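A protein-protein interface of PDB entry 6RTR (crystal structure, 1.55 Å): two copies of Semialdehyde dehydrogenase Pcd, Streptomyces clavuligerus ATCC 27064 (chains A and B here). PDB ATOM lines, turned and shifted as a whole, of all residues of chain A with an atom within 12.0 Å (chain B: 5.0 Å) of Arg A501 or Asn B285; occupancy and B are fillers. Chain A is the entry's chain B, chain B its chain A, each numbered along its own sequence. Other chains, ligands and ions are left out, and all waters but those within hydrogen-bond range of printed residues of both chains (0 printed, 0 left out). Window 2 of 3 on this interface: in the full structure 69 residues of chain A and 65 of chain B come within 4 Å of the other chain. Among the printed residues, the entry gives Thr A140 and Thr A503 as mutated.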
ATOM      1  N   THR A 140      25.973 -22.542 -17.173  1.00  0.00           N
ATOM      2  CA  THR A 140      25.701 -21.106 -17.002  1.00  0.00           C
ATOM      3  C   THR A 140      25.794 -20.755 -15.535  1.00  0.00           C
ATOM      4  O   THR A 140      25.488 -21.595 -14.654  1.00  0.00           O
ATOM      5  CB  THR A 140      24.307 -20.723 -17.565  1.00  0.00           C
ATOM      6  OG1 THR A 140      23.932 -19.450 -17.009  1.00  0.00           O
ATOM      7  CG2 THR A 140      23.287 -21.729 -17.200  1.00  0.00           C
ATOM      8  N   GLU A 141      26.172 -19.513 -15.253  1.00  0.00           N
ATOM      9  CA  GLU A 141      26.186 -18.991 -13.893  1.00  0.00           C
ATOM     10  C   GLU A 141      24.804 -18.746 -13.285  1.00  0.00           C
ATOM     11  O   GLU A 141      24.704 -18.504 -12.102  1.00  0.00           O
ATOM     12  CB  GLU A 141      27.066 -17.728 -13.804  1.00  0.00           C
ATOM     13  CG  GLU A 141      26.477 -16.498 -14.482  1.00  0.00           C
ATOM     14  CD  GLU A 141      27.425 -15.319 -14.417  1.00  0.00           C
ATOM     15  OE1 GLU A 141      28.526 -15.447 -14.964  1.00  0.00           O
ATOM     16  OE2 GLU A 141      27.085 -14.297 -13.766  1.00  0.00           O
ATOM     17  N   ARG A 142      23.760 -18.787 -14.127  1.00  0.00           N
ATOM     18  CA  ARG A 142      22.427 -18.399 -13.741  1.00  0.00           C
ATOM     19  C   ARG A 142      21.604 -19.655 -13.310  1.00  0.00           C
ATOM     20  O   ARG A 142      21.483 -20.608 -14.069  1.00  0.00           O
ATOM     21  CB  ARG A 142      21.689 -17.730 -14.924  1.00  0.00           C
ATOM     22  CG  ARG A 142      22.403 -16.537 -15.565  1.00  0.00           C
ATOM     23  CD  ARG A 142      21.732 -16.150 -16.869  1.00  0.00           C
ATOM     24  NE  ARG A 142      22.538 -15.225 -17.649  1.00  0.00           N
ATOM     25  CZ  ARG A 142      22.538 -13.907 -17.477  1.00  0.00           C
ATOM     26  NH1 ARG A 142      21.754 -13.344 -16.564  1.00  0.00           N
ATOM     27  NH2 ARG A 142      23.350 -13.138 -18.198  1.00  0.00           N
ATOM     28  N   PRO A 143      21.060 -19.658 -12.091  1.00  0.00           N
ATOM     29  CA  PRO A 143      20.240 -20.759 -11.683  1.00  0.00           C
ATOM     30  C   PRO A 143      19.028 -21.007 -12.604  1.00  0.00           C
ATOM     31  O   PRO A 143      18.393 -20.065 -13.014  1.00  0.00           O
ATOM     32  CB  PRO A 143      19.788 -20.345 -10.270  1.00  0.00           C
ATOM     33  CG  PRO A 143      20.847 -19.437  -9.778  1.00  0.00           C
ATOM     34  CD  PRO A 143      21.292 -18.685 -10.996  1.00  0.00           C
ATOM     35  N   GLY A 144      18.721 -22.245 -12.920  1.00  0.00           N
ATOM     36  CA  GLY A 144      17.506 -22.512 -13.695  1.00  0.00           C
ATOM     37  C   GLY A 144      17.586 -22.019 -15.127  1.00  0.00           C
ATOM     38  O   GLY A 144      16.554 -21.790 -15.764  1.00  0.00           O
ATOM     39  N   HIS A 145      18.794 -21.937 -15.668  1.00  0.00           N
ATOM     40  CA  HIS A 145      19.063 -21.620 -17.046  1.00  0.00           C
ATOM     41  C   HIS A 145      19.962 -22.710 -17.638  1.00  0.00           C
ATOM     42  O   HIS A 145      20.630 -23.485 -16.896  1.00  0.00           O
ATOM     43  CB  HIS A 145      19.765 -20.282 -17.201  1.00  0.00           C
ATOM     44  CG  HIS A 145      18.977 -19.068 -16.797  1.00  0.00           C
ATOM     45  ND1 HIS A 145      18.436 -18.893 -15.545  1.00  0.00           N
ATOM     46  CD2 HIS A 145      18.715 -17.924 -17.465  1.00  0.00           C
ATOM     47  CE1 HIS A 145      17.863 -17.696 -15.472  1.00  0.00           C
ATOM     48  NE2 HIS A 145      18.041 -17.087 -16.616  1.00  0.00           N
ATOM     49  N   ARG A 146      20.011 -22.765 -18.963  1.00  0.00           N
ATOM     50  CA  ARG A 146      20.907 -23.668 -19.696  1.00  0.00           C
ATOM     51  C   ARG A 146      21.602 -22.830 -20.758  1.00  0.00           C
ATOM     52  O   ARG A 146      21.035 -21.855 -21.271  1.00  0.00           O
ATOM     53  CB  ARG A 146      20.043 -24.756 -20.348  1.00  0.00           C
ATOM     54  CG  ARG A 146      20.808 -25.866 -21.000  1.00  0.00           C
ATOM     55  CD  ARG A 146      19.961 -27.007 -21.517  1.00  0.00           C
ATOM     56  NE  ARG A 146      18.936 -26.570 -22.469  1.00  0.00           N
ATOM     57  CZ  ARG A 146      19.167 -26.316 -23.761  1.00  0.00           C
ATOM     58  NH1 ARG A 146      20.399 -26.391 -24.261  1.00  0.00           N
ATOM     59  NH2 ARG A 146      18.148 -25.952 -24.554  1.00  0.00           N
ATOM     60  N   THR A 495      21.161 -18.835 -24.600  1.00  0.00           N
ATOM     61  CA  THR A 495      20.849 -18.993 -23.136  1.00  0.00           C
ATOM     62  C   THR A 495      19.344 -19.202 -23.047  1.00  0.00           C
ATOM     63  O   THR A 495      18.569 -18.437 -23.651  1.00  0.00           O
ATOM     64  CB  THR A 495      21.236 -17.774 -22.293  1.00  0.00           C
ATOM     65  OG1 THR A 495      22.671 -17.524 -22.421  1.00  0.00           O
ATOM     66  CG2 THR A 495      20.882 -17.950 -20.774  1.00  0.00           C
ATOM     67  N   VAL A 496      18.954 -20.258 -22.319  1.00  0.00           N
ATOM     68  CA  VAL A 496      17.550 -20.635 -22.168  1.00  0.00           C
ATOM     69  C   VAL A 496      17.208 -20.556 -20.695  1.00  0.00           C
ATOM     70  O   VAL A 496      17.823 -21.235 -19.865  1.00  0.00           O
ATOM     71  CB  VAL A 496      17.343 -22.042 -22.715  1.00  0.00           C
ATOM     72  CG1 VAL A 496      15.967 -22.550 -22.384  1.00  0.00           C
ATOM     73  CG2 VAL A 496      17.605 -22.020 -24.211  1.00  0.00           C
ATOM     74  N   ASN A 497      16.231 -19.728 -20.357  1.00  0.00           N
ATOM     75  CA  ASN A 497      15.716 -19.618 -18.993  1.00  0.00           C
ATOM     76  C   ASN A 497      14.506 -20.478 -18.838  1.00  0.00           C
ATOM     77  O   ASN A 497      13.531 -20.303 -19.593  1.00  0.00           O
ATOM     78  CB  ASN A 497      15.347 -18.154 -18.717  1.00  0.00           C
ATOM     79  CG  ASN A 497      14.841 -17.898 -17.299  1.00  0.00           C
ATOM     80  OD1 ASN A 497      14.963 -18.719 -16.385  1.00  0.00           O
ATOM     81  ND2 ASN A 497      14.264 -16.685 -17.112  1.00  0.00           N
ATOM     82  N   TYR A 498      14.524 -21.391 -17.890  1.00  0.00           N
ATOM     83  CA  TYR A 498      13.354 -22.211 -17.589  1.00  0.00           C
ATOM     84  C   TYR A 498      12.888 -22.021 -16.150  1.00  0.00           C
ATOM     85  O   TYR A 498      12.046 -22.779 -15.698  1.00  0.00           O
ATOM     86  CB  TYR A 498      13.638 -23.685 -17.914  1.00  0.00           C
ATOM     87  CG  TYR A 498      14.776 -24.325 -17.163  1.00  0.00           C
ATOM     88  CD1 TYR A 498      14.560 -24.983 -15.962  1.00  0.00           C
ATOM     89  CD2 TYR A 498      16.033 -24.357 -17.694  1.00  0.00           C
ATOM     90  CE1 TYR A 498      15.603 -25.594 -15.278  1.00  0.00           C
ATOM     91  CE2 TYR A 498      17.079 -24.972 -17.020  1.00  0.00           C
ATOM     92  CZ  TYR A 498      16.851 -25.565 -15.817  1.00  0.00           C
ATOM     93  OH  TYR A 498      17.899 -26.159 -15.174  1.00  0.00           O
ATOM     94  N   SER A 499      13.379 -20.988 -15.471  1.00  0.00           N
ATOM     95  CA  SER A 499      13.130 -20.712 -14.080  1.00  0.00           C
ATOM     96  C   SER A 499      11.898 -19.843 -13.863  1.00  0.00           C
ATOM     97  O   SER A 499      11.455 -19.795 -12.738  1.00  0.00           O
ATOM     98  CB  SER A 499      14.318 -19.986 -13.451  1.00  0.00           C
ATOM     99  OG  SER A 499      14.348 -18.599 -13.811  1.00  0.00           O
ATOM    100  N   GLY A 500      11.407 -19.148 -14.877  1.00  0.00           N
ATOM    101  CA  GLY A 500      10.351 -18.139 -14.712  1.00  0.00           C
ATOM    102  C   GLY A 500      10.729 -16.852 -13.972  1.00  0.00           C
ATOM    103  O   GLY A 500       9.853 -16.046 -13.693  1.00  0.00           O
ATOM    104  N   ARG A 501      12.015 -16.625 -13.696  1.00  0.00           N
ATOM    105  CA  ARG A 501      12.479 -15.464 -12.928  1.00  0.00           C
ATOM    106  C   ARG A 501      13.597 -14.747 -13.729  1.00  0.00           C
ATOM    107  O   ARG A 501      14.253 -15.378 -14.565  1.00  0.00           O
ATOM    108  CB  ARG A 501      12.972 -15.928 -11.547  1.00  0.00           C
ATOM    109  CG  ARG A 501      13.122 -14.830 -10.485  1.00  0.00           C
ATOM    110  CD  ARG A 501      11.801 -14.224  -9.960  1.00  0.00           C
ATOM    111  NE  ARG A 501      11.084 -13.436 -10.977  1.00  0.00           N
ATOM    112  CZ  ARG A 501      11.437 -12.231 -11.438  1.00  0.00           C
ATOM    113  NH1 ARG A 501      12.516 -11.599 -10.980  1.00  0.00           N
ATOM    114  NH2 ARG A 501      10.694 -11.646 -12.381  1.00  0.00           N
ATOM    115  N   VAL A 502      13.786 -13.441 -13.504  1.00  0.00           N
ATOM    116  CA  VAL A 502      14.889 -12.690 -14.106  1.00  0.00           C
ATOM    117  C   VAL A 502      16.111 -12.724 -13.166  1.00  0.00           C
ATOM    118  O   VAL A 502      16.111 -12.061 -12.119  1.00  0.00           O
ATOM    119  CB  VAL A 502      14.543 -11.211 -14.427  1.00  0.00           C
ATOM    120  CG1 VAL A 502      15.677 -10.521 -15.219  1.00  0.00           C
ATOM    121  CG2 VAL A 502      13.246 -11.073 -15.189  1.00  0.00           C
ATOM    122  N   THR A 503      17.135 -13.501 -13.560  1.00  0.00           N
ATOM    123  CA  THR A 503      18.461 -13.522 -12.907  1.00  0.00           C
ATOM    124  C   THR A 503      19.529 -12.902 -13.818  1.00  0.00           C
ATOM    125  O   THR A 503      19.917 -13.516 -14.823  1.00  0.00           O
ATOM    126  CB  THR A 503      18.916 -14.972 -12.596  1.00  0.00           C
ATOM    127  OG1 THR A 503      17.971 -15.601 -11.720  1.00  0.00           O
ATOM    128  CG2 THR A 503      20.329 -14.993 -11.956  1.00  0.00           C
ATOM    129  N   LEU A 504      20.031 -11.717 -13.441  1.00  0.00           N
ATOM    130  CA  LEU A 504      21.051 -11.010 -14.237  1.00  0.00           C
ATOM    131  C   LEU A 504      22.461 -11.490 -13.907  1.00  0.00           C
ATOM    132  O   LEU A 504      22.713 -11.973 -12.787  1.00  0.00           O
ATOM    133  CB  LEU A 504      20.937  -9.499 -14.024  1.00  0.00           C
ATOM    134  CG  LEU A 504      19.542  -8.907 -14.311  1.00  0.00           C
ATOM    135  CD1 LEU A 504      19.547  -7.389 -14.073  1.00  0.00           C
ATOM    136  CD2 LEU A 504      19.073  -9.260 -15.725  1.00  0.00           C
ATOM    137  N   ALA A 505      23.376 -11.361 -14.868  1.00  0.00           N
ATOM    138  CA  ALA A 505      24.771 -11.784 -14.649  1.00  0.00           C
ATOM    139  C   ALA A 505      25.503 -10.706 -13.839  1.00  0.00           C
ATOM    140  O   ALA A 505      26.457 -11.021 -13.117  1.00  0.00           O
ATOM    141  CB  ALA A 505      25.493 -12.058 -15.968  1.00  0.00           C
ATOM    142  N   LEU B 280       3.986 -12.430 -18.554  1.00  0.00           N
ATOM    143  CA  LEU B 280       4.112 -10.969 -18.696  1.00  0.00           C
ATOM    144  C   LEU B 280       4.875 -10.270 -17.585  1.00  0.00           C
ATOM    145  O   LEU B 280       5.597  -9.315 -17.854  1.00  0.00           O
ATOM    146  CB  LEU B 280       2.752 -10.315 -18.926  1.00  0.00           C
ATOM    147  CG  LEU B 280       2.079 -10.779 -20.221  1.00  0.00           C
ATOM    148  CD1 LEU B 280       0.820  -9.955 -20.438  1.00  0.00           C
ATOM    149  CD2 LEU B 280       2.970 -10.709 -21.450  1.00  0.00           C
ATOM    150  N   ASP B 281       4.779 -10.758 -16.364  1.00  0.00           N
ATOM    151  CA  ASP B 281       5.601 -10.221 -15.285  1.00  0.00           C
ATOM    152  C   ASP B 281       7.106 -10.417 -15.583  1.00  0.00           C
ATOM    153  O   ASP B 281       7.892  -9.453 -15.521  1.00  0.00           O
ATOM    154  CB  ASP B 281       5.241 -10.890 -13.954  1.00  0.00           C
ATOM    155  CG  ASP B 281       3.895 -10.395 -13.389  1.00  0.00           C
ATOM    156  OD1 ASP B 281       3.507 -10.901 -12.327  1.00  0.00           O
ATOM    157  OD2 ASP B 281       3.250  -9.512 -13.990  1.00  0.00           O
ATOM    158  N   LEU B 282       7.467 -11.644 -15.974  1.00  0.00           N
ATOM    159  CA  LEU B 282       8.844 -11.920 -16.368  1.00  0.00           C
ATOM    160  C   LEU B 282       9.239 -11.014 -17.536  1.00  0.00           C
ATOM    161  O   LEU B 282      10.301 -10.378 -17.508  1.00  0.00           O
ATOM    162  CB  LEU B 282       9.021 -13.398 -16.726  1.00  0.00           C
ATOM    163  CG  LEU B 282      10.327 -13.713 -17.477  1.00  0.00           C
ATOM    164  CD1 LEU B 282      11.442 -13.591 -16.499  1.00  0.00           C
ATOM    165  CD2 LEU B 282      10.263 -15.093 -18.109  1.00  0.00           C
ATOM    166  N   THR B 283       8.405 -10.962 -18.563  1.00  0.00           N
ATOM    167  CA  THR B 283       8.715 -10.227 -19.772  1.00  0.00           C
ATOM    168  C   THR B 283       8.928  -8.722 -19.549  1.00  0.00           C
ATOM    169  O   THR B 283       9.866  -8.112 -20.071  1.00  0.00           O
ATOM    170  CB  THR B 283       7.618 -10.469 -20.843  1.00  0.00           C
ATOM    171  OG1 THR B 283       7.556 -11.885 -21.096  1.00  0.00           O
ATOM    172  CG2 THR B 283       7.900  -9.775 -22.147  1.00  0.00           C
ATOM    173  N   VAL B 284       8.033  -8.115 -18.769  1.00  0.00           N
ATOM    174  CA  VAL B 284       8.130  -6.704 -18.552  1.00  0.00           C
ATOM    175  C   VAL B 284       9.384  -6.388 -17.775  1.00  0.00           C
ATOM    176  O   VAL B 284      10.093  -5.455 -18.158  1.00  0.00           O
ATOM    177  CB  VAL B 284       6.847  -6.163 -17.875  1.00  0.00           C
ATOM    178  CG1 VAL B 284       7.074  -4.712 -17.408  1.00  0.00           C
ATOM    179  CG2 VAL B 284       5.706  -6.217 -18.862  1.00  0.00           C
ATOM    180  N   ASN B 285       9.669  -7.150 -16.732  1.00  0.00           N
ATOM    181  CA  ASN B 285      10.889  -6.958 -15.956  1.00  0.00           C
ATOM    182  C   ASN B 285      12.118  -7.097 -16.848  1.00  0.00           C
ATOM    183  O   ASN B 285      12.986  -6.247 -16.826  1.00  0.00           O
ATOM    184  CB  ASN B 285      10.985  -7.880 -14.761  1.00  0.00           C
ATOM    185  CG  ASN B 285      10.052  -7.455 -13.644  1.00  0.00           C
ATOM    186  OD1 ASN B 285       9.792  -6.274 -13.460  1.00  0.00           O
ATOM    187  ND2 ASN B 285       9.537  -8.415 -12.907  1.00  0.00           N
ATOM    188  N   ALA B 286      12.166  -8.165 -17.646  1.00  0.00           N
ATOM    189  CA  ALA B 286      13.317  -8.381 -18.498  1.00  0.00           C
ATOM    190  C   ALA B 286      13.484  -7.276 -19.544  1.00  0.00           C
ATOM    191  O   ALA B 286      14.608  -6.784 -19.770  1.00  0.00           O
ATOM    192  CB  ALA B 286      13.231  -9.756 -19.154  1.00  0.00           C
ATOM    193  N   ALA B 287      12.378  -6.863 -20.153  1.00  0.00           N
ATOM    194  CA  ALA B 287      12.411  -5.861 -21.176  1.00  0.00           C
ATOM    195  C   ALA B 287      12.843  -4.526 -20.607  1.00  0.00           C
ATOM    196  O   ALA B 287      13.619  -3.822 -21.229  1.00  0.00           O
ATOM    197  CB  ALA B 287      11.056  -5.741 -21.852  1.00  0.00           C
ATOM    198  N   VAL B 288      12.372  -4.172 -19.415  1.00  0.00           N
ATOM    199  CA  VAL B 288      12.755  -2.881 -18.856  1.00  0.00           C
ATOM    200  C   VAL B 288      14.262  -2.831 -18.583  1.00  0.00           C
ATOM    201  O   VAL B 288      14.954  -1.875 -18.984  1.00  0.00           O
ATOM    202  CB  VAL B 288      11.943  -2.532 -17.576  1.00  0.00           C
ATOM    203  CG1 VAL B 288      12.529  -1.310 -16.859  1.00  0.00           C
ATOM    204  CG2 VAL B 288      10.496  -2.289 -17.913  1.00  0.00           C
ATOM    205  N   PHE B 289      14.806  -3.865 -17.949  1.00  0.00           N
ATOM    206  CA  PHE B 289      16.254  -3.926 -17.708  1.00  0.00           C
ATOM    207  C   PHE B 289      17.030  -3.854 -18.997  1.00  0.00           C
ATOM    208  O   PHE B 289      17.996  -3.111 -19.105  1.00  0.00           O
ATOM    209  CB  PHE B 289      16.714  -5.204 -16.973  1.00  0.00           C
ATOM    210  CG  PHE B 289      18.244  -5.460 -17.033  1.00  0.00           C
ATOM    211  CD1 PHE B 289      19.138  -4.670 -16.287  1.00  0.00           C
ATOM    212  CD2 PHE B 289      18.801  -6.496 -17.838  1.00  0.00           C
ATOM    213  CE1 PHE B 289      20.511  -4.937 -16.306  1.00  0.00           C
ATOM    214  CE2 PHE B 289      20.164  -6.736 -17.877  1.00  0.00           C
ATOM    215  CZ  PHE B 289      21.028  -5.959 -17.114  1.00  0.00           C
ATOM    216  N   ARG B 325       7.812   4.782 -13.990  1.00  0.00           N
ATOM    217  CA  ARG B 325       8.291   4.625 -12.622  1.00  0.00           C
ATOM    218  C   ARG B 325       9.808   4.490 -12.516  1.00  0.00           C
ATOM    219  O   ARG B 325      10.333   4.360 -11.412  1.00  0.00           O
ATOM    220  CB  ARG B 325       7.585   3.468 -11.884  1.00  0.00           C
ATOM    221  CG  ARG B 325       7.751   2.066 -12.470  1.00  0.00           C
ATOM    222  CD  ARG B 325       8.145   0.931 -11.501  1.00  0.00           C
ATOM    223  NE  ARG B 325       8.265  -0.406 -12.157  1.00  0.00           N
ATOM    224  CZ  ARG B 325       9.233  -0.796 -13.012  1.00  0.00           C
ATOM    225  NH1 ARG B 325      10.212   0.035 -13.388  1.00  0.00           N
ATOM    226  NH2 ARG B 325       9.217  -2.042 -13.513  1.00  0.00           N
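ND2 of Asn B285 sits close to NH2 of Arg A501, 3.5 Å away.
The backbone carbonyl oxygen (O) of Asp B281 is in hydrogen-bond range of the side-chain amide nitrogen (ND2) of Asn B285 (3.3 Å).
The backbone carbonyl oxygen (O) of Arg A501 is in hydrogen-bond range of the side-chain amide nitrogen (ND2) of Asn A497 (2.9 Å).
The side-chain hydroxyl of Ser A499 is in hydrogen-bond range of the backbone NH of Arg A501, 3.1 Å away.
Arg A501 touches Leu B282 (C to CD1, 3.7 Å).
Val A502 touches Leu B282.
Asn B285 touches Val A502 (CB to CG2, 3.9 Å).
Ala B286 touches Val A502.
CE1 of Phe B289 touches CD1 of Leu A504, 3.5 Å away.
Thr A140 touches none of the printed residues of chain B.
Of the printed residues of chain B, Arg A501 touches Leu B282 (3.7 Å) and Asn B285 (3.5 Å).
Of the printed residues of chain B, Val A502 touches Leu B282 (3.4 Å), Asn B285 (3.9 Å) and Ala B286 (3.96 Å).
Thr A503 touches none of the printed residues of chain B.
Printed residues of chain B within 4 Å of Leu A504: Phe B289.
No residue of chain A comes within 4 Å of Thr B283.
No residue of chain A comes within 4 Å of Val B284.
Of chain A, only Arg A501 (3.5 Å) and Val A502 (3.9 Å) come within 4 Å of Asn B285.
Ala B287 touches none of the printed residues of chain A.
Val B288 touches none of the printed residues of chain A.
Of the printed residues of chain A, Phe B289 touches Leu A504.
The nearest residue of chain A that does not touch Asn B285 is Leu A504 (6.9 Å).
The nearest printed residue of chain B that does not touch Val A502 is Asp B281 (5.6 Å).
Of the 11 printed residues of chain B, 4 touch a printed residue of chain A.
Printed residues of chain B that touch a printed residue of chain A: Leu B282, Asn B285, Ala B286 and Phe B289.
Hydrophobic or aromatic side chains of chain B within 4 Å of the printed part of chain A: Leu B282 and Phe B289.
Of the 18 printed residues of chain A, 3 touch a printed residue of chain B.
Hydrophobic or aromatic side chains of chain A within 4 Å of the printed part of chain B: Val A502 and Leu A504.
Among the printed residues, no Asp or Glu carboxylate lies within 4 Å of a Lys or Arg side-chain nitrogen of the other chain.
No position is printed for both chains.
Of the 6 pairs that touch across the chains among the printed residues, none has its exchanged pair printed and touching as well.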
